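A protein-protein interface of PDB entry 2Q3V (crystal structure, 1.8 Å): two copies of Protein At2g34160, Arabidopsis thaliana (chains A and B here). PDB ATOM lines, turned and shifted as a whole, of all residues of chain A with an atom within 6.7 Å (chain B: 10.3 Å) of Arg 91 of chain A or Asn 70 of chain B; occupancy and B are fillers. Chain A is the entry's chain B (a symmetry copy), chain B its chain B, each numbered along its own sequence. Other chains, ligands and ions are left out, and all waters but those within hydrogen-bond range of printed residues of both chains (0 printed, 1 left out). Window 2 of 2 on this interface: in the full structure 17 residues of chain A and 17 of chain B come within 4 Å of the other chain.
The guanidinium group (NH1) of Arg 91 of chain A sits at hydrogen-bond distance from the side-chain amide oxygen (OD1) of Asn 70 of chain B, 3.4 Å away. NZ of Lys 97 of chain A is in salt-bridge range of OE1 of Glu 66 of chain B, at 3.2 Å. The side-chain amide oxygen of Asn 70 of chain B is in hydrogen-bond range of the backbone NH of Gln 96 of chain A (2.8 Å).
NZ of Lys 69 of chain B lies within salt-bridge range of OE1 of Glu 76 of chain B, 2.9 Å away. The backbone carbonyl oxygen (O) of Glu 66 of chain B lies within hydrogen-bond range of the side-chain amide nitrogen (ND2) of Asn 70 of chain B (2.8 Å). OD1 of Asp 88 of chain A lies within hydrogen-bond range of N of Arg 91 of chain A (2.6 Å).
Val 95 of chain A touches Asn 70 of chain B. Gln 96 of chain A touches Lys 69 of chain B (OE1 to CE, 2.9 Å).
Of chain B, only Asn 70 (3.4 Å) comes within 4 Å of Arg 91 of chain A. Of chain A, only Arg 91, Val 95 and Gln 96 come within 4 Å of Asn 70 of chain B. No residue of chain B comes within 4 Å of Asp 88 of chain A. Gly 92 of chain A touches none of the printed residues of chain B. Val 95 of chain A touches just one residue of chain B: Asn 70. Of the printed residues of chain B, Gln 96 of chain A touches Lys 69 (2.9 Å) and Asn 70 (2.8 Å). Of the printed residues of chain A, Glu 66 of chain B touches Lys 97 (3.2 Å). Of the printed residues of chain B, Lys 97 of chain A touches Glu 66 (3.2 Å). Printed residues of chain A within 4 Å of Lys 69 of chain B: Gln 96. Val 75 of chain B touches none of the printed residues of chain A. Asp 89 of chain A touches none of the printed residues of chain B. The nearest printed residue of chain A that does not touch Lys 69 of chain B is Arg 91 of chain A (6.4 Å).
Printed residues of chain B that touch a printed residue of chain A: Glu 66, Lys 69 and Asn 70. Of the 10 printed residues of chain A, 4 touch a printed residue of chain B. Among the printed residues, 5 pairs touch across the chains. Among the printed residues, Asp or Glu carboxylates within 4 Å of a Lys or Arg side-chain nitrogen of the other chain: Lys 97 of chain A with Glu 66 of chain B (3.2 Å).
No position is printed for both chains. Of the 5 pairs that touch across the chains among the printed residues, none has its exchanged pair printed and touching as well.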
ATOM      1  N   ASP A  88     -31.218 -22.903  29.544  1.00  0.00           N
ATOM      2  CA  ASP A  88     -31.236 -22.620  30.984  1.00  0.00           C
ATOM      3  C   ASP A  88     -32.671 -22.527  31.548  1.00  0.00           C
ATOM      4  O   ASP A  88     -33.241 -21.437  31.656  1.00  0.00           O
ATOM      5  CB  ASP A  88     -30.495 -21.308  31.258  1.00  0.00           C
ATOM      6  CG  ASP A  88     -30.406 -20.982  32.744  1.00  0.00           C
ATOM      7  OD1 ASP A  88     -31.398 -21.208  33.456  1.00  0.00           O
ATOM      8  OD2 ASP A  88     -29.354 -20.489  33.198  1.00  0.00           O
ATOM      9  N   ASP A  89     -33.240 -23.667  31.918  1.00  0.00           N
ATOM     10  CA  ASP A  89     -34.612 -23.689  32.430  1.00  0.00           C
ATOM     11  C   ASP A  89     -34.852 -22.701  33.592  1.00  0.00           C
ATOM     12  O   ASP A  89     -35.911 -22.092  33.687  1.00  0.00           O
ATOM     13  CB  ASP A  89     -34.984 -25.126  32.829  1.00  0.00           C
ATOM     14  CG  ASP A  89     -34.916 -26.100  31.640  1.00  0.00           C
ATOM     15  OD1 ASP A  89     -35.424 -25.755  30.561  1.00  0.00           O
ATOM     16  OD2 ASP A  89     -34.362 -27.212  31.779  1.00  0.00           O
ATOM     17  N   ALA A  90     -33.859 -22.501  34.446  1.00  0.00           N
ATOM     18  CA  ALA A  90     -34.014 -21.587  35.584  1.00  0.00           C
ATOM     19  C   ALA A  90     -34.161 -20.126  35.164  1.00  0.00           C
ATOM     20  O   ALA A  90     -35.015 -19.411  35.687  1.00  0.00           O
ATOM     21  CB  ALA A  90     -32.827 -21.733  36.544  1.00  0.00           C
ATOM     22  N   ARG A  91     -33.321 -19.671  34.234  1.00  0.00           N
ATOM     23  CA  ARG A  91     -33.410 -18.280  33.809  1.00  0.00           C
ATOM     24  C   ARG A  91     -34.520 -18.057  32.784  1.00  0.00           C
ATOM     25  O   ARG A  91     -34.774 -16.918  32.346  1.00  0.00           O
ATOM     26  CB  ARG A  91     -32.074 -17.802  33.245  1.00  0.00           C
ATOM     27  CG  ARG A  91     -32.035 -16.305  33.005  1.00  0.00           C
ATOM     28  CD  ARG A  91     -30.677 -15.881  32.507  1.00  0.00           C
ATOM     29  NE  ARG A  91     -30.609 -14.454  32.220  1.00  0.00           N
ATOM     30  CZ  ARG A  91     -29.523 -13.850  31.753  1.00  0.00           C
ATOM     31  NH1 ARG A  91     -28.424 -14.557  31.523  1.00  0.00           N
ATOM     32  NH2 ARG A  91     -29.532 -12.545  31.520  1.00  0.00           N
ATOM     33  N   GLY A  92     -35.191 -19.141  32.404  1.00  0.00           N
ATOM     34  CA  GLY A  92     -36.270 -19.025  31.437  1.00  0.00           C
ATOM     35  C   GLY A  92     -35.850 -18.923  29.982  1.00  0.00           C
ATOM     36  O   GLY A  92     -36.516 -19.476  29.101  1.00  0.00           O
ATOM     37  N   ARG A  93     -34.759 -18.192  29.732  1.00  0.00           N
ATOM     38  CA  ARG A  93     -34.192 -17.998  28.400  1.00  0.00           C
ATOM     39  C   ARG A  93     -32.716 -18.333  28.568  1.00  0.00           C
ATOM     40  O   ARG A  93     -32.153 -18.079  29.625  1.00  0.00           O
ATOM     41  CB  ARG A  93     -34.360 -16.545  27.923  1.00  0.00           C
ATOM     42  CG  ARG A  93     -33.746 -15.482  28.821  1.00  0.00           C
ATOM     43  CD  ARG A  93     -33.985 -14.095  28.236  1.00  0.00           C
ATOM     44  NE  ARG A  93     -33.618 -13.002  29.138  1.00  0.00           N
ATOM     45  CZ  ARG A  93     -34.210 -12.756  30.304  1.00  0.00           C
ATOM     46  NH1 ARG A  93     -35.205 -13.530  30.726  1.00  0.00           N
ATOM     47  NH2 ARG A  93     -33.814 -11.729  31.047  1.00  0.00           N
ATOM     48  N   PRO A  94     -32.076 -18.899  27.528  1.00  0.00           N
ATOM     49  CA  PRO A  94     -30.654 -19.294  27.550  1.00  0.00           C
ATOM     50  C   PRO A  94     -29.653 -18.246  28.021  1.00  0.00           C
ATOM     51  O   PRO A  94     -29.829 -17.068  27.775  1.00  0.00           O
ATOM     52  CB  PRO A  94     -30.393 -19.737  26.104  1.00  0.00           C
ATOM     53  CG  PRO A  94     -31.748 -20.252  25.671  1.00  0.00           C
ATOM     54  CD  PRO A  94     -32.679 -19.193  26.216  1.00  0.00           C
ATOM     55  N   VAL A  95     -28.598 -18.674  28.710  1.00  0.00           N
ATOM     56  CA  VAL A  95     -27.585 -17.714  29.158  1.00  0.00           C
ATOM     57  C   VAL A  95     -26.468 -17.865  28.139  1.00  0.00           C
ATOM     58  O   VAL A  95     -26.601 -18.653  27.191  1.00  0.00           O
ATOM     59  CB  VAL A  95     -27.053 -18.016  30.606  1.00  0.00           C
ATOM     60  CG1 VAL A  95     -28.206 -17.983  31.581  1.00  0.00           C
ATOM     61  CG2 VAL A  95     -26.357 -19.351  30.659  1.00  0.00           C
ATOM     62  N   GLN A  96     -25.385 -17.119  28.306  1.00  0.00           N
ATOM     63  CA  GLN A  96     -24.287 -17.244  27.370  1.00  0.00           C
ATOM     64  C   GLN A  96     -23.028 -17.698  28.092  1.00  0.00           C
ATOM     65  O   GLN A  96     -22.775 -17.278  29.220  1.00  0.00           O
ATOM     66  CB  GLN A  96     -24.044 -15.915  26.687  1.00  0.00           C
ATOM     67  CG  GLN A  96     -25.156 -15.556  25.729  1.00  0.00           C
ATOM     68  CD  GLN A  96     -24.941 -14.190  25.160  1.00  0.00           C
ATOM     69  OE1 GLN A  96     -23.943 -13.946  24.496  1.00  0.00           O
ATOM     70  NE2 GLN A  96     -25.869 -13.275  25.435  1.00  0.00           N
ATOM     71  N   LYS A  97     -22.251 -18.586  27.454  1.00  0.00           N
ATOM     72  CA  LYS A  97     -21.007 -19.053  28.069  1.00  0.00           C
ATOM     73  C   LYS A  97     -19.876 -19.062  27.073  1.00  0.00           C
ATOM     74  O   LYS A  97     -20.097 -19.165  25.867  1.00  0.00           O
ATOM     75  CB  LYS A  97     -21.150 -20.498  28.586  1.00  0.00           C
ATOM     76  CG  LYS A  97     -22.073 -20.668  29.807  1.00  0.00           C
ATOM     77  CD  LYS A  97     -21.477 -19.961  31.043  1.00  0.00           C
ATOM     78  CE  LYS A  97     -20.244 -20.706  31.598  1.00  0.00           C
ATOM     79  NZ  LYS A  97     -19.709 -20.025  32.831  1.00  0.00           N
ATOM     80  N   VAL B  36     -13.935  -5.786  34.791  1.00  0.00           N
ATOM     81  CA  VAL B  36     -15.268  -5.602  34.224  1.00  0.00           C
ATOM     82  C   VAL B  36     -15.576  -4.090  34.112  1.00  0.00           C
ATOM     83  O   VAL B  36     -16.036  -3.601  33.064  1.00  0.00           O
ATOM     84  CB  VAL B  36     -16.392  -6.271  35.103  1.00  0.00           C
ATOM     85  CG1 VAL B  36     -17.794  -6.105  34.438  1.00  0.00           C
ATOM     86  CG2 VAL B  36     -16.103  -7.765  35.284  1.00  0.00           C
ATOM     87  N   LYS B  40     -16.033  -1.644  30.972  1.00  0.00           N
ATOM     88  CA  LYS B  40     -17.235  -0.802  30.801  1.00  0.00           C
ATOM     89  C   LYS B  40     -16.816   0.636  30.455  1.00  0.00           C
ATOM     90  O   LYS B  40     -17.404   1.281  29.569  1.00  0.00           O
ATOM     91  CB  LYS B  40     -18.106  -0.809  32.073  1.00  0.00           C
ATOM     92  CG  LYS B  40     -18.979  -2.077  32.216  1.00  0.00           C
ATOM     93  CD  LYS B  40     -19.780  -2.017  33.518  1.00  0.00           C
ATOM     94  CE  LYS B  40     -20.591  -3.263  33.745  1.00  0.00           C
ATOM     95  NZ  LYS B  40     -21.248  -3.243  35.100  1.00  0.00           N
ATOM     96  N   VAL B  62     -12.468 -14.566  30.175  1.00  0.00           N
ATOM     97  CA  VAL B  62     -13.624 -15.406  29.845  1.00  0.00           C
ATOM     98  C   VAL B  62     -14.811 -14.962  30.719  1.00  0.00           C
ATOM     99  O   VAL B  62     -15.917 -14.715  30.214  1.00  0.00           O
ATOM    100  CB  VAL B  62     -13.281 -16.907  30.107  1.00  0.00           C
ATOM    101  CG1 VAL B  62     -14.563 -17.742  30.262  1.00  0.00           C
ATOM    102  CG2 VAL B  62     -12.436 -17.426  28.951  1.00  0.00           C
ATOM    103  N   THR B  63     -14.559 -14.823  32.022  1.00  0.00           N
ATOM    104  CA  THR B  63     -15.611 -14.422  32.962  1.00  0.00           C
ATOM    105  C   THR B  63     -16.084 -12.988  32.726  1.00  0.00           C
ATOM    106  O   THR B  63     -17.277 -12.693  32.831  1.00  0.00           O
ATOM    107  CB  THR B  63     -15.150 -14.581  34.426  1.00  0.00           C
ATOM    108  OG1 THR B  63     -14.794 -15.953  34.658  1.00  0.00           O
ATOM    109  CG2 THR B  63     -16.287 -14.222  35.382  1.00  0.00           C
ATOM    110  N   VAL B  64     -15.167 -12.088  32.412  1.00  0.00           N
ATOM    111  CA  VAL B  64     -15.584 -10.697  32.137  1.00  0.00           C
ATOM    112  C   VAL B  64     -16.555 -10.659  30.939  1.00  0.00           C
ATOM    113  O   VAL B  64     -17.612 -10.015  30.972  1.00  0.00           O
ATOM    114  CB  VAL B  64     -14.348  -9.810  31.811  1.00  0.00           C
ATOM    115  CG1 VAL B  64     -14.794  -8.426  31.228  1.00  0.00           C
ATOM    116  CG2 VAL B  64     -13.507  -9.646  33.067  1.00  0.00           C
ATOM    117  N   THR B  65     -16.190 -11.359  29.867  1.00  0.00           N
ATOM    118  CA  THR B  65     -17.043 -11.385  28.693  1.00  0.00           C
ATOM    119  C   THR B  65     -18.408 -11.988  28.977  1.00  0.00           C
ATOM    120  O   THR B  65     -19.419 -11.477  28.508  1.00  0.00           O
ATOM    121  CB  THR B  65     -16.380 -12.186  27.558  1.00  0.00           C
ATOM    122  OG1 THR B  65     -15.209 -11.485  27.127  1.00  0.00           O
ATOM    123  CG2 THR B  65     -17.343 -12.361  26.389  1.00  0.00           C
ATOM    124  N   GLU B  66     -18.431 -13.084  29.728  1.00  0.00           N
ATOM    125  CA  GLU B  66     -19.696 -13.725  30.065  1.00  0.00           C
ATOM    126  C   GLU B  66     -20.540 -12.753  30.862  1.00  0.00           C
ATOM    127  O   GLU B  66     -21.740 -12.629  30.646  1.00  0.00           O
ATOM    128  CB  GLU B  66     -19.447 -14.997  30.878  1.00  0.00           C
ATOM    129  CG  GLU B  66     -18.777 -16.091  29.996  1.00  0.00           C
ATOM    130  CD  GLU B  66     -18.486 -17.391  30.746  1.00  0.00           C
ATOM    131  OE1 GLU B  66     -18.210 -17.349  31.975  1.00  0.00           O
ATOM    132  OE2 GLU B  66     -18.477 -18.466  30.099  1.00  0.00           O
ATOM    133  N   ILE B  67     -19.911 -12.079  31.810  1.00  0.00           N
ATOM    134  CA  ILE B  67     -20.652 -11.104  32.588  1.00  0.00           C
ATOM    135  C   ILE B  67     -21.192  -9.992  31.704  1.00  0.00           C
ATOM    136  O   ILE B  67     -22.409  -9.734  31.699  1.00  0.00           O
ATOM    137  CB  ILE B  67     -19.778 -10.520  33.691  1.00  0.00           C
ATOM    138  CG1 ILE B  67     -19.549 -11.629  34.753  1.00  0.00           C
ATOM    139  CG2 ILE B  67     -20.448  -9.260  34.324  1.00  0.00           C
ATOM    140  CD1 ILE B  67     -18.431 -11.290  35.746  1.00  0.00           C
ATOM    141  N   LEU B  68     -20.318  -9.331  30.956  1.00  0.00           N
ATOM    142  CA  LEU B  68     -20.783  -8.213  30.124  1.00  0.00           C
ATOM    143  C   LEU B  68     -21.848  -8.667  29.146  1.00  0.00           C
ATOM    144  O   LEU B  68     -22.867  -8.017  29.023  1.00  0.00           O
ATOM    145  CB  LEU B  68     -19.608  -7.575  29.356  1.00  0.00           C
ATOM    146  CG  LEU B  68     -18.608  -6.912  30.321  1.00  0.00           C
ATOM    147  CD1 LEU B  68     -17.327  -6.544  29.556  1.00  0.00           C
ATOM    148  CD2 LEU B  68     -19.222  -5.659  30.976  1.00  0.00           C
ATOM    149  N   LYS B  69     -21.615  -9.785  28.448  1.00  0.00           N
ATOM    150  CA  LYS B  69     -22.631 -10.277  27.504  1.00  0.00           C
ATOM    151  C   LYS B  69     -23.983 -10.585  28.165  1.00  0.00           C
ATOM    152  O   LYS B  69     -25.054 -10.167  27.695  1.00  0.00           O
ATOM    153  CB  LYS B  69     -22.152 -11.576  26.831  1.00  0.00           C
ATOM    154  CG  LYS B  69     -21.043 -11.415  25.802  1.00  0.00           C
ATOM    155  CD  LYS B  69     -21.520 -10.706  24.522  1.00  0.00           C
ATOM    156  CE  LYS B  69     -22.871 -11.273  24.060  1.00  0.00           C
ATOM    157  NZ  LYS B  69     -23.245 -10.838  22.697  1.00  0.00           N
ATOM    158  N   ASN B  70     -23.941 -11.372  29.232  1.00  0.00           N
ATOM    159  CA  ASN B  70     -25.162 -11.774  29.903  1.00  0.00           C
ATOM    160  C   ASN B  70     -25.933 -10.604  30.470  1.00  0.00           C
ATOM    161  O   ASN B  70     -27.118 -10.450  30.155  1.00  0.00           O
ATOM    162  CB  ASN B  70     -24.877 -12.803  31.001  1.00  0.00           C
ATOM    163  CG  ASN B  70     -24.679 -14.198  30.434  1.00  0.00           C
ATOM    164  OD1 ASN B  70     -25.543 -14.723  29.710  1.00  0.00           O
ATOM    165  ND2 ASN B  70     -23.538 -14.797  30.736  1.00  0.00           N
ATOM    166  N   ASN B  71     -25.289  -9.782  31.286  1.00  0.00           N
ATOM    167  CA  ASN B  71     -26.014  -8.653  31.867  1.00  0.00           C
ATOM    168  C   ASN B  71     -26.525  -7.713  30.771  1.00  0.00           C
ATOM    169  O   ASN B  71     -27.421  -6.897  31.004  1.00  0.00           O
ATOM    170  CB  ASN B  71     -25.180  -7.938  32.966  1.00  0.00           C
ATOM    171  CG  ASN B  71     -25.304  -8.617  34.371  1.00  0.00           C
ATOM    172  OD1 ASN B  71     -24.503  -8.329  35.310  1.00  0.00           O
ATOM    173  ND2 ASN B  71     -26.285  -9.509  34.523  1.00  0.00           N
ATOM    174  N   GLY B  72     -25.964  -7.806  29.562  1.00  0.00           N
ATOM    175  CA  GLY B  72     -26.528  -7.020  28.473  1.00  0.00           C
ATOM    176  C   GLY B  72     -25.775  -5.835  27.959  1.00  0.00           C
ATOM    177  O   GLY B  72     -26.258  -5.108  27.068  1.00  0.00           O
ATOM    178  N   PHE B  73     -24.578  -5.649  28.495  1.00  0.00           N
ATOM    179  CA  PHE B  73     -23.765  -4.511  28.116  1.00  0.00           C
ATOM    180  C   PHE B  73     -23.127  -4.567  26.762  1.00  0.00           C
ATOM    181  O   PHE B  73     -23.077  -3.560  26.055  1.00  0.00           O
ATOM    182  CB  PHE B  73     -22.674  -4.286  29.182  1.00  0.00           C
ATOM    183  CG  PHE B  73     -23.217  -3.802  30.486  1.00  0.00           C
ATOM    184  CD1 PHE B  73     -23.491  -2.441  30.670  1.00  0.00           C
ATOM    185  CD2 PHE B  73     -23.502  -4.696  31.520  1.00  0.00           C
ATOM    186  CE1 PHE B  73     -24.041  -1.960  31.877  1.00  0.00           C
ATOM    187  CE2 PHE B  73     -24.049  -4.221  32.731  1.00  0.00           C
ATOM    188  CZ  PHE B  73     -24.315  -2.839  32.893  1.00  0.00           C
ATOM    189  N   ALA B  74     -22.638  -5.738  26.366  1.00  0.00           N
ATOM    190  CA  ALA B  74     -21.922  -5.784  25.110  1.00  0.00           C
ATOM    191  C   ALA B  74     -22.159  -7.005  24.265  1.00  0.00           C
ATOM    192  O   ALA B  74     -22.820  -7.974  24.686  1.00  0.00           O
ATOM    193  CB  ALA B  74     -20.422  -5.656  25.366  1.00  0.00           C
ATOM    194  N   VAL B  75     -21.604  -6.923  23.068  1.00  0.00           N
ATOM    195  CA  VAL B  75     -21.649  -8.006  22.090  1.00  0.00           C
ATOM    196  C   VAL B  75     -20.186  -8.221  21.683  1.00  0.00           C
ATOM    197  O   VAL B  75     -19.364  -7.278  21.656  1.00  0.00           O
ATOM    198  CB  VAL B  75     -22.482  -7.605  20.849  1.00  0.00           C
ATOM    199  CG1 VAL B  75     -22.588  -8.785  19.874  1.00  0.00           C
ATOM    200  CG2 VAL B  75     -23.877  -7.176  21.297  1.00  0.00           C
ATOM    201  N   GLU B  76     -19.820  -9.462  21.406  1.00  0.00           N
ATOM    202  CA  GLU B  76     -18.447  -9.717  21.002  1.00  0.00           C
ATOM    203  C   GLU B  76     -18.311  -9.595  19.472  1.00  0.00           C
ATOM    204  O   GLU B  76     -19.202  -9.999  18.731  1.00  0.00           O
ATOM    205  CB  GLU B  76     -18.010 -11.135  21.432  1.00  0.00           C
ATOM    206  CG  GLU B  76     -18.578 -12.292  20.597  1.00  0.00           C
ATOM    207  CD  GLU B  76     -20.075 -12.583  20.807  1.00  0.00           C
ATOM    208  OE1 GLU B  76     -20.776 -11.851  21.560  1.00  0.00           O
ATOM    209  OE2 GLU B  76     -20.553 -13.577  20.204  1.00  0.00           O
ATOM    210  N   LEU B 104     -14.740  -6.449  22.361  1.00  0.00           N
ATOM    211  CA  LEU B 104     -16.169  -6.290  22.639  1.00  0.00           C
ATOM    212  C   LEU B 104     -16.546  -4.879  22.219  1.00  0.00           C
ATOM    213  O   LEU B 104     -15.696  -3.981  22.206  1.00  0.00           O
ATOM    214  CB  LEU B 104     -16.457  -6.422  24.144  1.00  0.00           C
ATOM    215  CG  LEU B 104     -15.968  -7.719  24.831  1.00  0.00           C
ATOM    216  CD1 LEU B 104     -16.280  -7.621  26.348  1.00  0.00           C
ATOM    217  CD2 LEU B 104     -16.662  -8.944  24.200  1.00  0.00           C
ATOM    218  N   SER B 107     -23.256  -2.607  23.406  1.00  0.00           N
ATOM    219  CA  SER B 107     -24.530  -3.124  22.892  1.00  0.00           C
ATOM    220  C   SER B 107     -25.510  -1.955  22.840  1.00  0.00           C
ATOM    221  O   SER B 107     -25.229  -0.903  23.409  1.00  0.00           O
ATOM    222  CB  SER B 107     -25.130  -4.159  23.837  1.00  0.00           C
ATOM    223  OG  SER B 107     -25.741  -3.526  24.950  1.00  0.00           O
ATOM    224  N   LYS B 109     -28.184  -1.808  24.397  1.00  0.00           N
ATOM    225  CA  LYS B 109     -28.745  -1.633  25.742  1.00  0.00           C
ATOM    226  C   LYS B 109     -27.745  -1.018  26.739  1.00  0.00           C
ATOM    227  O   LYS B 109     -28.122  -0.688  27.874  1.00  0.00           O
ATOM    228  CB  LYS B 109     -29.226  -2.981  26.316  1.00  0.00           C
ATOM    229  CG  LYS B 109     -30.595  -3.464  25.782  1.00  0.00           C
ATOM    230  CD  LYS B 109     -31.683  -2.440  26.065  1.00  0.00           C
ATOM    231  CE  LYS B 109     -33.032  -2.846  25.482  1.00  0.00           C
ATOM    232  NZ  LYS B 109     -34.069  -1.811  25.782  1.00  0.00           N
ATOM    233  N   LEU B 113     -28.537   0.625  30.539  1.00  0.00           N
ATOM    234  CA  LEU B 113     -28.039  -0.090  31.722  1.00  0.00           C
ATOM    235  C   LEU B 113     -27.079   0.767  32.546  1.00  0.00           C
ATOM    236  O   LEU B 113     -27.079   0.696  33.780  1.00  0.00           O
ATOM    237  CB  LEU B 113     -27.302  -1.372  31.302  1.00  0.00           C
ATOM    238  CG  LEU B 113     -28.137  -2.493  30.686  1.00  0.00           C
ATOM    239  CD1 LEU B 113     -27.194  -3.596  30.185  1.00  0.00           C
ATOM    240  CD2 LEU B 113     -29.116  -3.052  31.717  1.00  0.00           C
